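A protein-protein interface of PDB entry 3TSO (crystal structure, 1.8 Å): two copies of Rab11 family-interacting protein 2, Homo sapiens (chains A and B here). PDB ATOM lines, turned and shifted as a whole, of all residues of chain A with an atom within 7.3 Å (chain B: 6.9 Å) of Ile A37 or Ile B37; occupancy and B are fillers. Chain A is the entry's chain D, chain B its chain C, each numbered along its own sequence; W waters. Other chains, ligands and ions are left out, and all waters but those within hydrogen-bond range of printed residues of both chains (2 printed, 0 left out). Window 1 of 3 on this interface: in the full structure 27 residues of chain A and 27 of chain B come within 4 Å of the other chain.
The side-chain amino group of Lys B33 lies within salt-bridge range of the side-chain carboxylate of Asp A34 (2.9 Å).
OD1 of Asp B34 is in salt-bridge range of NZ of Lys A33 (2.9 Å).
Among the printed residues, pairs that only touch across the chains: Leu A30 with Leu B30, Ile A44 with Ile B44, Ile A37 with Ile B37, Lys A33 with Leu B30, His A36 with Glu B41, Leu A40 with Ile B44, Ile A44 with Leu B40, Leu A30 with Lys B33, Tyr A43 with Ile B44, Ile A44 with Tyr B43, Ile A37 with Leu B40, Leu A40 with Ile B37, Leu A40 with Leu B40 and Leu A40 with Glu B41.
Of the printed residues of chain B, Ile A37 touches Ile B37 (3.4 Å) and Leu B40 (3.9 Å).
Of chain A, only Ile A37 and Leu A40 come within 4 Å of Ile B37.
Printed residues of chain B within 4 Å of His A36: Glu B41 (3.7 Å).
Printed residues of chain A within 4 Å of Leu B30: Leu A30 and Lys A33.
Of the printed residues of chain A, Tyr B43 touches Ile A44 (3.8 Å).
Of the printed residues of chain B, Ile A44 touches Leu B40 (3.7 Å), Tyr B43 (3.8 Å) and Ile B44 (3.4 Å).
Printed residues of chain A within 4 Å of Asp B34: Lys A33.
The nearest residue of chain B that does not touch Ile A37 is Lys B33 (4.1 Å).
Of the 14 printed residues of chain B, 8 touch a printed residue of chain A.
Of the 15 printed residues of chain A, 8 touch a printed residue of chain B.
Among the printed residues, Asp or Glu carboxylates within 4 Å of a Lys or Arg side-chain nitrogen of the other chain: Lys A33 with Asp B34 and Asp A34 with Lys B33.
Ile A37 touches its own counterpart, Ile B37.
Leu A40 touches Ile B44, and with the chains exchanged Ile A44 touches Leu B40.
Tyr A43 touches Ile B44, and with the chains exchanged Ile A44 touches Tyr B43.
Ile B44 touches its own counterpart, Ile A44.
Of the 16 pairs that touch across the chains among the printed residues, 14 have their exchanged pair printed and touching as well.
Water W1 lies within hydrogen-bond range of the side-chain carboxylate (OE2) of Glu A41 (2.6 Å) and a ring nitrogen (NE2) of His B36 (3.4 Å).
Water W2 bridges OE2 of Glu A41 (2.7 Å) and ND1 of His B36 (3.2 Å).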
ATOM      1  N   LEU A  30       2.701  -0.422   2.302  1.00  0.00           N
ATOM      2  CA  LEU A  30       2.660  -1.724   1.598  1.00  0.00           C
ATOM      3  C   LEU A  30       2.382  -1.655   0.119  1.00  0.00           C
ATOM      4  O   LEU A  30       3.018  -2.364  -0.673  1.00  0.00           O
ATOM      5  CB  LEU A  30       1.610  -2.632   2.172  1.00  0.00           C
ATOM      6  CG  LEU A  30       1.895  -3.335   3.460  1.00  0.00           C
ATOM      7  CD1 LEU A  30       0.956  -4.558   3.399  1.00  0.00           C
ATOM      8  CD2 LEU A  30       3.378  -3.767   3.516  1.00  0.00           C
ATOM      9  N   ARG A  31       1.411  -0.821  -0.270  1.00  0.00           N
ATOM     10  CA  ARG A  31       1.147  -0.672  -1.691  1.00  0.00           C
ATOM     11  C   ARG A  31       2.390  -0.194  -2.428  1.00  0.00           C
ATOM     12  O   ARG A  31       2.666  -0.687  -3.546  1.00  0.00           O
ATOM     13  CB  ARG A  31      -0.035   0.285  -1.969  1.00  0.00           C
ATOM     14  CG  ARG A  31      -1.388  -0.347  -1.692  1.00  0.00           C
ATOM     15  N   ARG A  32       3.107   0.775  -1.862  1.00  0.00           N
ATOM     16  CA  ARG A  32       4.320   1.305  -2.564  1.00  0.00           C
ATOM     17  C   ARG A  32       5.460   0.280  -2.621  1.00  0.00           C
ATOM     18  O   ARG A  32       6.266   0.303  -3.563  1.00  0.00           O
ATOM     19  CB  ARG A  32       4.870   2.604  -1.945  1.00  0.00           C
ATOM     20  CG  ARG A  32       3.822   3.799  -1.999  1.00  0.00           C
ATOM     21  CD  ARG A  32       4.382   5.096  -1.499  1.00  0.00           C
ATOM     22  NE  ARG A  32       4.537   5.079  -0.037  1.00  0.00           N
ATOM     23  CZ  ARG A  32       3.885   5.903   0.795  1.00  0.00           C
ATOM     24  NH1 ARG A  32       3.071   6.837   0.284  1.00  0.00           N
ATOM     25  NH2 ARG A  32       4.047   5.818   2.128  1.00  0.00           N
ATOM     26  N   LYS A  33       5.549  -0.548  -1.593  1.00  0.00           N
ATOM     27  CA  LYS A  33       6.596  -1.573  -1.514  1.00  0.00           C
ATOM     28  C   LYS A  33       6.323  -2.682  -2.561  1.00  0.00           C
ATOM     29  O   LYS A  33       7.244  -3.164  -3.229  1.00  0.00           O
ATOM     30  CB  LYS A  33       6.743  -2.080  -0.056  1.00  0.00           C
ATOM     31  CG  LYS A  33       7.566  -1.038   0.828  1.00  0.00           C
ATOM     32  CD  LYS A  33       8.023  -1.521   2.162  1.00  0.00           C
ATOM     33  CE  LYS A  33       8.812  -0.394   2.946  1.00  0.00           C
ATOM     34  NZ  LYS A  33       9.945   0.258   2.143  1.00  0.00           N
ATOM     35  N   ASP A  34       5.055  -3.010  -2.733  1.00  0.00           N
ATOM     36  CA  ASP A  34       4.612  -3.959  -3.750  1.00  0.00           C
ATOM     37  C   ASP A  34       4.889  -3.465  -5.176  1.00  0.00           C
ATOM     38  O   ASP A  34       5.366  -4.207  -6.021  1.00  0.00           O
ATOM     39  CB  ASP A  34       3.106  -4.313  -3.561  1.00  0.00           C
ATOM     40  CG  ASP A  34       2.879  -5.394  -2.518  1.00  0.00           C
ATOM     41  OD1 ASP A  34       3.807  -6.148  -2.169  1.00  0.00           O
ATOM     42  OD2 ASP A  34       1.760  -5.505  -1.969  1.00  0.00           O
ATOM     43  N   THR A  35       4.575  -2.201  -5.450  1.00  0.00           N
ATOM     44  CA  THR A  35       4.922  -1.623  -6.722  1.00  0.00           C
ATOM     45  C   THR A  35       6.441  -1.651  -6.920  1.00  0.00           C
ATOM     46  O   THR A  35       6.878  -1.989  -7.976  1.00  0.00           O
ATOM     47  CB  THR A  35       4.421  -0.193  -6.765  1.00  0.00           C
ATOM     48  OG1 THR A  35       3.043  -0.280  -6.461  1.00  0.00           O
ATOM     49  CG2 THR A  35       4.626   0.450  -8.155  1.00  0.00           C
ATOM     50  N   HIS A  36       7.213  -1.236  -5.922  1.00  0.00           N
ATOM     51  CA  HIS A  36       8.664  -1.247  -6.045  1.00  0.00           C
ATOM     52  C   HIS A  36       9.181  -2.679  -6.311  1.00  0.00           C
ATOM     53  O   HIS A  36      10.031  -2.858  -7.171  1.00  0.00           O
ATOM     54  CB  HIS A  36       9.353  -0.610  -4.826  1.00  0.00           C
ATOM     55  CG  HIS A  36      10.813  -0.408  -5.029  1.00  0.00           C
ATOM     56  ND1 HIS A  36      11.335   0.011  -6.233  1.00  0.00           N
ATOM     57  CD2 HIS A  36      11.866  -0.582  -4.202  1.00  0.00           C
ATOM     58  CE1 HIS A  36      12.648   0.097  -6.137  1.00  0.00           C
ATOM     59  NE2 HIS A  36      12.997  -0.280  -4.926  1.00  0.00           N
ATOM     60  N   ILE A  37       8.702  -3.669  -5.577  1.00  0.00           N
ATOM     61  CA  ILE A  37       9.085  -5.070  -5.835  1.00  0.00           C
ATOM     62  C   ILE A  37       8.837  -5.486  -7.290  1.00  0.00           C
ATOM     63  O   ILE A  37       9.687  -6.111  -7.944  1.00  0.00           O
ATOM     64  CB  ILE A  37       8.385  -6.034  -4.878  1.00  0.00           C
ATOM     65  CG1 ILE A  37       8.956  -5.875  -3.456  1.00  0.00           C
ATOM     66  CG2 ILE A  37       8.474  -7.546  -5.354  1.00  0.00           C
ATOM     67  CD1 ILE A  37       8.092  -6.550  -2.396  1.00  0.00           C
ATOM     68  N   ARG A  38       7.677  -5.095  -7.819  1.00  0.00           N
ATOM     69  CA  ARG A  38       7.429  -5.487  -9.185  1.00  0.00           C
ATOM     70  C   ARG A  38       8.328  -4.715 -10.138  1.00  0.00           C
ATOM     71  O   ARG A  38       8.746  -5.295 -11.157  1.00  0.00           O
ATOM     72  CB  ARG A  38       5.905  -5.351  -9.528  1.00  0.00           C
ATOM     73  CG  ARG A  38       5.610  -5.679 -10.991  1.00  0.00           C
ATOM     74  CD  ARG A  38       5.857  -7.192 -11.307  1.00  0.00           C
ATOM     75  NE  ARG A  38       4.577  -7.902 -11.249  1.00  0.00           N
ATOM     76  CZ  ARG A  38       3.911  -8.336 -12.316  1.00  0.00           C
ATOM     77  NH1 ARG A  38       4.403  -8.172 -13.547  1.00  0.00           N
ATOM     78  NH2 ARG A  38       2.758  -8.954 -12.134  1.00  0.00           N
ATOM     79  N   GLU A  39       8.670  -3.464  -9.821  1.00  0.00           N
ATOM     80  CA  GLU A  39       9.612  -2.714 -10.657  1.00  0.00           C
ATOM     81  C   GLU A  39      10.976  -3.405 -10.722  1.00  0.00           C
ATOM     82  O   GLU A  39      11.569  -3.503 -11.776  1.00  0.00           O
ATOM     83  CB  GLU A  39       9.786  -1.239 -10.180  1.00  0.00           C
ATOM     84  CG  GLU A  39       8.510  -0.400 -10.613  1.00  0.00           C
ATOM     85  CD  GLU A  39       8.258   0.898  -9.816  1.00  0.00           C
ATOM     86  OE1 GLU A  39       8.924   1.100  -8.763  1.00  0.00           O
ATOM     87  OE2 GLU A  39       7.378   1.691 -10.265  1.00  0.00           O
ATOM     88  N   LEU A  40      11.422  -3.872  -9.568  1.00  0.00           N
ATOM     89  CA  LEU A  40      12.710  -4.594  -9.428  1.00  0.00           C
ATOM     90  C   LEU A  40      12.661  -5.918 -10.220  1.00  0.00           C
ATOM     91  O   LEU A  40      13.597  -6.253 -10.929  1.00  0.00           O
ATOM     92  CB  LEU A  40      12.957  -4.831  -7.914  1.00  0.00           C
ATOM     93  CG  LEU A  40      13.385  -3.635  -7.065  1.00  0.00           C
ATOM     94  CD1 LEU A  40      13.379  -4.098  -5.598  1.00  0.00           C
ATOM     95  CD2 LEU A  40      14.806  -3.114  -7.402  1.00  0.00           C
ATOM     96  N   GLU A  41      11.554  -6.651 -10.109  1.00  0.00           N
ATOM     97  CA  GLU A  41      11.340  -7.941 -10.831  1.00  0.00           C
ATOM     98  C   GLU A  41      11.328  -7.749 -12.356  1.00  0.00           C
ATOM     99  O   GLU A  41      12.004  -8.503 -13.078  1.00  0.00           O
ATOM    100  CB  GLU A  41      10.046  -8.631 -10.376  1.00  0.00           C
ATOM    101  CG  GLU A  41      10.188  -9.181  -8.896  1.00  0.00           C
ATOM    102  CD  GLU A  41       8.874  -9.673  -8.327  1.00  0.00           C
ATOM    103  OE1 GLU A  41       7.816  -9.246  -8.839  1.00  0.00           O
ATOM    104  OE2 GLU A  41       8.896 -10.494  -7.387  1.00  0.00           O
ATOM    105  N   ASP A  42      10.626  -6.711 -12.815  1.00  0.00           N
ATOM    106  CA  ASP A  42      10.620  -6.367 -14.225  1.00  0.00           C
ATOM    107  C   ASP A  42      12.011  -5.937 -14.763  1.00  0.00           C
ATOM    108  O   ASP A  42      12.427  -6.377 -15.824  1.00  0.00           O
ATOM    109  CB  ASP A  42       9.630  -5.248 -14.488  1.00  0.00           C
ATOM    110  CG  ASP A  42       8.185  -5.735 -14.452  1.00  0.00           C
ATOM    111  OD1 ASP A  42       7.887  -6.956 -14.237  1.00  0.00           O
ATOM    112  OD2 ASP A  42       7.387  -4.825 -14.506  1.00  0.00           O
ATOM    113  N   TYR A  43      12.708  -5.087 -14.008  1.00  0.00           N
ATOM    114  CA  TYR A  43      14.089  -4.745 -14.328  1.00  0.00           C
ATOM    115  C   TYR A  43      14.917  -6.040 -14.491  1.00  0.00           C
ATOM    116  O   TYR A  43      15.722  -6.148 -15.451  1.00  0.00           O
ATOM    117  CB  TYR A  43      14.735  -3.919 -13.196  1.00  0.00           C
ATOM    118  CG  TYR A  43      16.168  -3.529 -13.527  1.00  0.00           C
ATOM    119  CD1 TYR A  43      17.229  -4.319 -13.107  1.00  0.00           C
ATOM    120  CD2 TYR A  43      16.460  -2.391 -14.318  1.00  0.00           C
ATOM    121  CE1 TYR A  43      18.537  -3.991 -13.400  1.00  0.00           C
ATOM    122  CE2 TYR A  43      17.817  -2.036 -14.608  1.00  0.00           C
ATOM    123  CZ  TYR A  43      18.830  -2.858 -14.141  1.00  0.00           C
ATOM    124  OH  TYR A  43      20.158  -2.578 -14.431  1.00  0.00           O
ATOM    125  N   ILE A  44      14.864  -6.941 -13.485  1.00  0.00           N
ATOM    126  CA  ILE A  44      15.606  -8.166 -13.541  1.00  0.00           C
ATOM    127  C   ILE A  44      15.310  -8.976 -14.789  1.00  0.00           C
ATOM    128  O   ILE A  44      16.240  -9.424 -15.502  1.00  0.00           O
ATOM    129  CB  ILE A  44      15.355  -9.016 -12.234  1.00  0.00           C
ATOM    130  CG1 ILE A  44      16.089  -8.329 -11.038  1.00  0.00           C
ATOM    131  CG2 ILE A  44      15.884 -10.447 -12.435  1.00  0.00           C
ATOM    132  CD1 ILE A  44      15.643  -8.900  -9.639  1.00  0.00           C
ATOM    133  N   LEU B  30       5.362  -5.830   6.223  1.00  0.00           N
ATOM    134  CA  LEU B  30       6.306  -4.777   5.833  1.00  0.00           C
ATOM    135  C   LEU B  30       7.754  -5.274   6.028  1.00  0.00           C
ATOM    136  O   LEU B  30       8.609  -5.026   5.186  1.00  0.00           O
ATOM    137  CB  LEU B  30       6.129  -3.508   6.664  1.00  0.00           C
ATOM    138  CG  LEU B  30       5.364  -2.280   6.196  1.00  0.00           C
ATOM    139  CD1 LEU B  30       5.681  -1.054   7.083  1.00  0.00           C
ATOM    140  CD2 LEU B  30       5.736  -1.888   4.730  1.00  0.00           C
ATOM    141  N   ARG B  32       8.906  -8.402   5.998  1.00  0.00           N
ATOM    142  CA  ARG B  32       9.139  -9.414   4.957  1.00  0.00           C
ATOM    143  C   ARG B  32       9.336  -8.734   3.608  1.00  0.00           C
ATOM    144  O   ARG B  32      10.222  -9.119   2.837  1.00  0.00           O
ATOM    145  CB  ARG B  32       7.964 -10.412   4.875  1.00  0.00           C
ATOM    146  CG  ARG B  32       7.813 -11.372   6.124  1.00  0.00           C
ATOM    147  CD  ARG B  32       6.650 -12.346   5.929  1.00  0.00           C
ATOM    148  NE  ARG B  32       6.340 -13.086   7.158  1.00  0.00           N
ATOM    149  CZ  ARG B  32       5.132 -13.146   7.738  1.00  0.00           C
ATOM    150  NH1 ARG B  32       4.059 -12.510   7.203  1.00  0.00           N
ATOM    151  NH2 ARG B  32       4.998 -13.854   8.869  1.00  0.00           N
ATOM    152  N   LYS B  33       8.538  -7.720   3.298  1.00  0.00           N
ATOM    153  CA  LYS B  33       8.649  -7.055   2.000  1.00  0.00           C
ATOM    154  C   LYS B  33       9.991  -6.309   1.856  1.00  0.00           C
ATOM    155  O   LYS B  33      10.664  -6.396   0.773  1.00  0.00           O
ATOM    156  CB  LYS B  33       7.383  -6.216   1.713  1.00  0.00           C
ATOM    157  CG  LYS B  33       6.189  -7.171   1.220  1.00  0.00           C
ATOM    158  CD  LYS B  33       4.770  -6.616   1.480  1.00  0.00           C
ATOM    159  CE  LYS B  33       3.653  -7.599   0.916  1.00  0.00           C
ATOM    160  NZ  LYS B  33       4.097  -8.369  -0.332  1.00  0.00           N
ATOM    161  N   ASP B  34      10.428  -5.681   2.963  1.00  0.00           N
ATOM    162  CA  ASP B  34      11.721  -4.952   3.019  1.00  0.00           C
ATOM    163  C   ASP B  34      12.892  -5.902   2.836  1.00  0.00           C
ATOM    164  O   ASP B  34      13.815  -5.603   2.066  1.00  0.00           O
ATOM    165  CB  ASP B  34      11.901  -4.143   4.340  1.00  0.00           C
ATOM    166  CG  ASP B  34      11.229  -2.754   4.258  1.00  0.00           C
ATOM    167  OD1 ASP B  34      10.820  -2.302   3.153  1.00  0.00           O
ATOM    168  OD2 ASP B  34      11.072  -2.099   5.302  1.00  0.00           O
ATOM    169  N   THR B  35      12.800  -7.054   3.502  1.00  0.00           N
ATOM    170  CA  THR B  35      13.765  -8.155   3.331  1.00  0.00           C
ATOM    171  C   THR B  35      13.864  -8.571   1.889  1.00  0.00           C
ATOM    172  O   THR B  35      14.978  -8.709   1.332  1.00  0.00           O
ATOM    173  CB  THR B  35      13.488  -9.409   4.263  1.00  0.00           C
ATOM    174  OG1 THR B  35      13.632  -9.034   5.638  1.00  0.00           O
ATOM    175  CG2 THR B  35      14.490 -10.595   4.002  1.00  0.00           C
ATOM    176  N   HIS B  36      12.715  -8.801   1.273  1.00  0.00           N
ATOM    177  CA  HIS B  36      12.763  -9.297  -0.084  1.00  0.00           C
ATOM    178  C   HIS B  36      13.189  -8.226  -1.091  1.00  0.00           C
ATOM    179  O   HIS B  36      13.924  -8.516  -2.046  1.00  0.00           O
ATOM    180  CB  HIS B  36      11.452  -9.952  -0.533  1.00  0.00           C
ATOM    181  CG  HIS B  36      11.625 -10.721  -1.810  1.00  0.00           C
ATOM    182  ND1 HIS B  36      10.851 -10.499  -2.930  1.00  0.00           N
ATOM    183  CD2 HIS B  36      12.550 -11.646  -2.162  1.00  0.00           C
ATOM    184  CE1 HIS B  36      11.274 -11.277  -3.913  1.00  0.00           C
ATOM    185  NE2 HIS B  36      12.297 -11.987  -3.470  1.00  0.00           N
ATOM    186  N   ILE B  37      12.840  -6.968  -0.835  1.00  0.00           N
ATOM    187  CA  ILE B  37      13.371  -5.867  -1.669  1.00  0.00           C
ATOM    188  C   ILE B  37      14.931  -5.889  -1.701  1.00  0.00           C
ATOM    189  O   ILE B  37      15.572  -5.716  -2.781  1.00  0.00           O
ATOM    190  CB  ILE B  37      12.851  -4.477  -1.174  1.00  0.00           C
ATOM    191  CG1 ILE B  37      11.359  -4.314  -1.601  1.00  0.00           C
ATOM    192  CG2 ILE B  37      13.618  -3.294  -1.772  1.00  0.00           C
ATOM    193  CD1 ILE B  37      10.629  -3.191  -0.737  1.00  0.00           C
ATOM    194  N   ARG B  38      15.504  -6.074  -0.506  1.00  0.00           N
ATOM    195  CA  ARG B  38      16.999  -6.077  -0.416  1.00  0.00           C
ATOM    196  C   ARG B  38      17.563  -7.315  -1.066  1.00  0.00           C
ATOM    197  O   ARG B  38      18.629  -7.232  -1.665  1.00  0.00           O
ATOM    198  CB  ARG B  38      17.498  -6.010   1.042  1.00  0.00           C
ATOM    199  CG  ARG B  38      19.045  -6.191   1.223  1.00  0.00           C
ATOM    200  CD  ARG B  38      19.835  -4.999   0.514  1.00  0.00           C
ATOM    201  NE  ARG B  38      19.544  -3.760   1.237  1.00  0.00           N
ATOM    202  CZ  ARG B  38      20.174  -3.393   2.348  1.00  0.00           C
ATOM    203  NH1 ARG B  38      21.195  -4.115   2.828  1.00  0.00           N
ATOM    204  NH2 ARG B  38      19.798  -2.297   2.952  1.00  0.00           N
ATOM    205  N   GLU B  39      16.890  -8.456  -0.929  1.00  0.00           N
ATOM    206  CA  GLU B  39      17.301  -9.657  -1.720  1.00  0.00           C
ATOM    207  C   GLU B  39      17.295  -9.347  -3.224  1.00  0.00           C
ATOM    208  O   GLU B  39      18.236  -9.739  -3.938  1.00  0.00           O
ATOM    209  CB  GLU B  39      16.443 -10.916  -1.407  1.00  0.00           C
ATOM    210  CG  GLU B  39      16.697 -11.478   0.013  1.00  0.00           C
ATOM    211  CD  GLU B  39      15.525 -12.290   0.536  1.00  0.00           C
ATOM    212  OE1 GLU B  39      14.453 -12.356  -0.147  1.00  0.00           O
ATOM    213  OE2 GLU B  39      15.709 -12.891   1.613  1.00  0.00           O
ATOM    214  N   LEU B  40      16.251  -8.694  -3.720  1.00  0.00           N
ATOM    215  CA  LEU B  40      16.201  -8.369  -5.193  1.00  0.00           C
ATOM    216  C   LEU B  40      17.285  -7.374  -5.609  1.00  0.00           C
ATOM    217  O   LEU B  40      17.942  -7.522  -6.669  1.00  0.00           O
ATOM    218  CB  LEU B  40      14.822  -7.768  -5.600  1.00  0.00           C
ATOM    219  CG  LEU B  40      13.739  -8.847  -5.517  1.00  0.00           C
ATOM    220  CD1 LEU B  40      12.314  -8.152  -5.540  1.00  0.00           C
ATOM    221  CD2 LEU B  40      13.832  -9.902  -6.586  1.00  0.00           C
ATOM    222  N   GLU B  41      17.501  -6.398  -4.753  1.00  0.00           N
ATOM    223  CA  GLU B  41      18.511  -5.337  -5.003  1.00  0.00           C
ATOM    224  C   GLU B  41      19.921  -5.936  -4.953  1.00  0.00           C
ATOM    225  O   GLU B  41      20.776  -5.570  -5.821  1.00  0.00           O
ATOM    226  CB  GLU B  41      18.379  -4.222  -3.970  1.00  0.00           C
ATOM    227  CG  GLU B  41      17.134  -3.365  -4.211  1.00  0.00           C
ATOM    228  CD  GLU B  41      16.906  -2.281  -3.169  1.00  0.00           C
ATOM    229  OE1 GLU B  41      17.443  -2.407  -2.057  1.00  0.00           O
ATOM    230  OE2 GLU B  41      16.197  -1.307  -3.487  1.00  0.00           O
ATOM    231  N   ASP B  42      20.175  -6.815  -3.984  1.00  0.00           N
ATOM    232  CA  ASP B  42      21.442  -7.559  -3.925  1.00  0.00           C
ATOM    233  C   ASP B  42      21.643  -8.491  -5.141  1.00  0.00           C
ATOM    234  O   ASP B  42      22.706  -8.487  -5.759  1.00  0.00           O
ATOM    235  CB  ASP B  42      21.577  -8.382  -2.648  1.00  0.00           C
ATOM    236  CG  ASP B  42      21.875  -7.536  -1.386  1.00  0.00           C
ATOM    237  OD1 ASP B  42      22.098  -6.313  -1.467  1.00  0.00           O
ATOM    238  OD2 ASP B  42      21.863  -8.176  -0.301  1.00  0.00           O
ATOM    239  N   TYR B  43      20.594  -9.218  -5.573  1.00  0.00           N
ATOM    240  CA  TYR B  43      20.724  -9.980  -6.789  1.00  0.00           C
ATOM    241  C   TYR B  43      21.159  -9.048  -7.974  1.00  0.00           C
ATOM    242  O   TYR B  43      22.130  -9.346  -8.714  1.00  0.00           O
ATOM    243  CB  TYR B  43      19.383 -10.674  -7.122  1.00  0.00           C
ATOM    244  CG  TYR B  43      19.461 -11.452  -8.389  1.00  0.00           C
ATOM    245  CD1 TYR B  43      19.025 -10.880  -9.590  1.00  0.00           C
ATOM    246  CD2 TYR B  43      20.065 -12.768  -8.395  1.00  0.00           C
ATOM    247  CE1 TYR B  43      19.163 -11.598 -10.812  1.00  0.00           C
ATOM    248  CE2 TYR B  43      20.178 -13.482  -9.530  1.00  0.00           C
ATOM    249  CZ  TYR B  43      19.697 -12.902 -10.778  1.00  0.00           C
ATOM    250  OH  TYR B  43      19.855 -13.610 -11.973  1.00  0.00           O
ATOM    251  N   ILE B  44      20.433  -7.957  -8.154  1.00  0.00           N
ATOM    252  CA  ILE B  44      20.693  -7.029  -9.237  1.00  0.00           C
ATOM    253  C   ILE B  44      22.182  -6.562  -9.190  1.00  0.00           C
ATOM    254  O   ILE B  44      22.917  -6.515 -10.220  1.00  0.00           O
ATOM    255  CB  ILE B  44      19.706  -5.832  -9.130  1.00  0.00           C
ATOM    256  CG1 ILE B  44      18.315  -6.291  -9.513  1.00  0.00           C
ATOM    257  CG2 ILE B  44      20.160  -4.593 -10.031  1.00  0.00           C
ATOM    258  CD1 ILE B  44      17.184  -5.243  -9.214  1.00  0.00           C
HETATM  259  O   HOH W   1      10.922 -11.979  -6.578  1.00  0.00           O
HETATM  260  O   HOH W   2       8.403 -11.126  -4.813  1.00  0.00           O
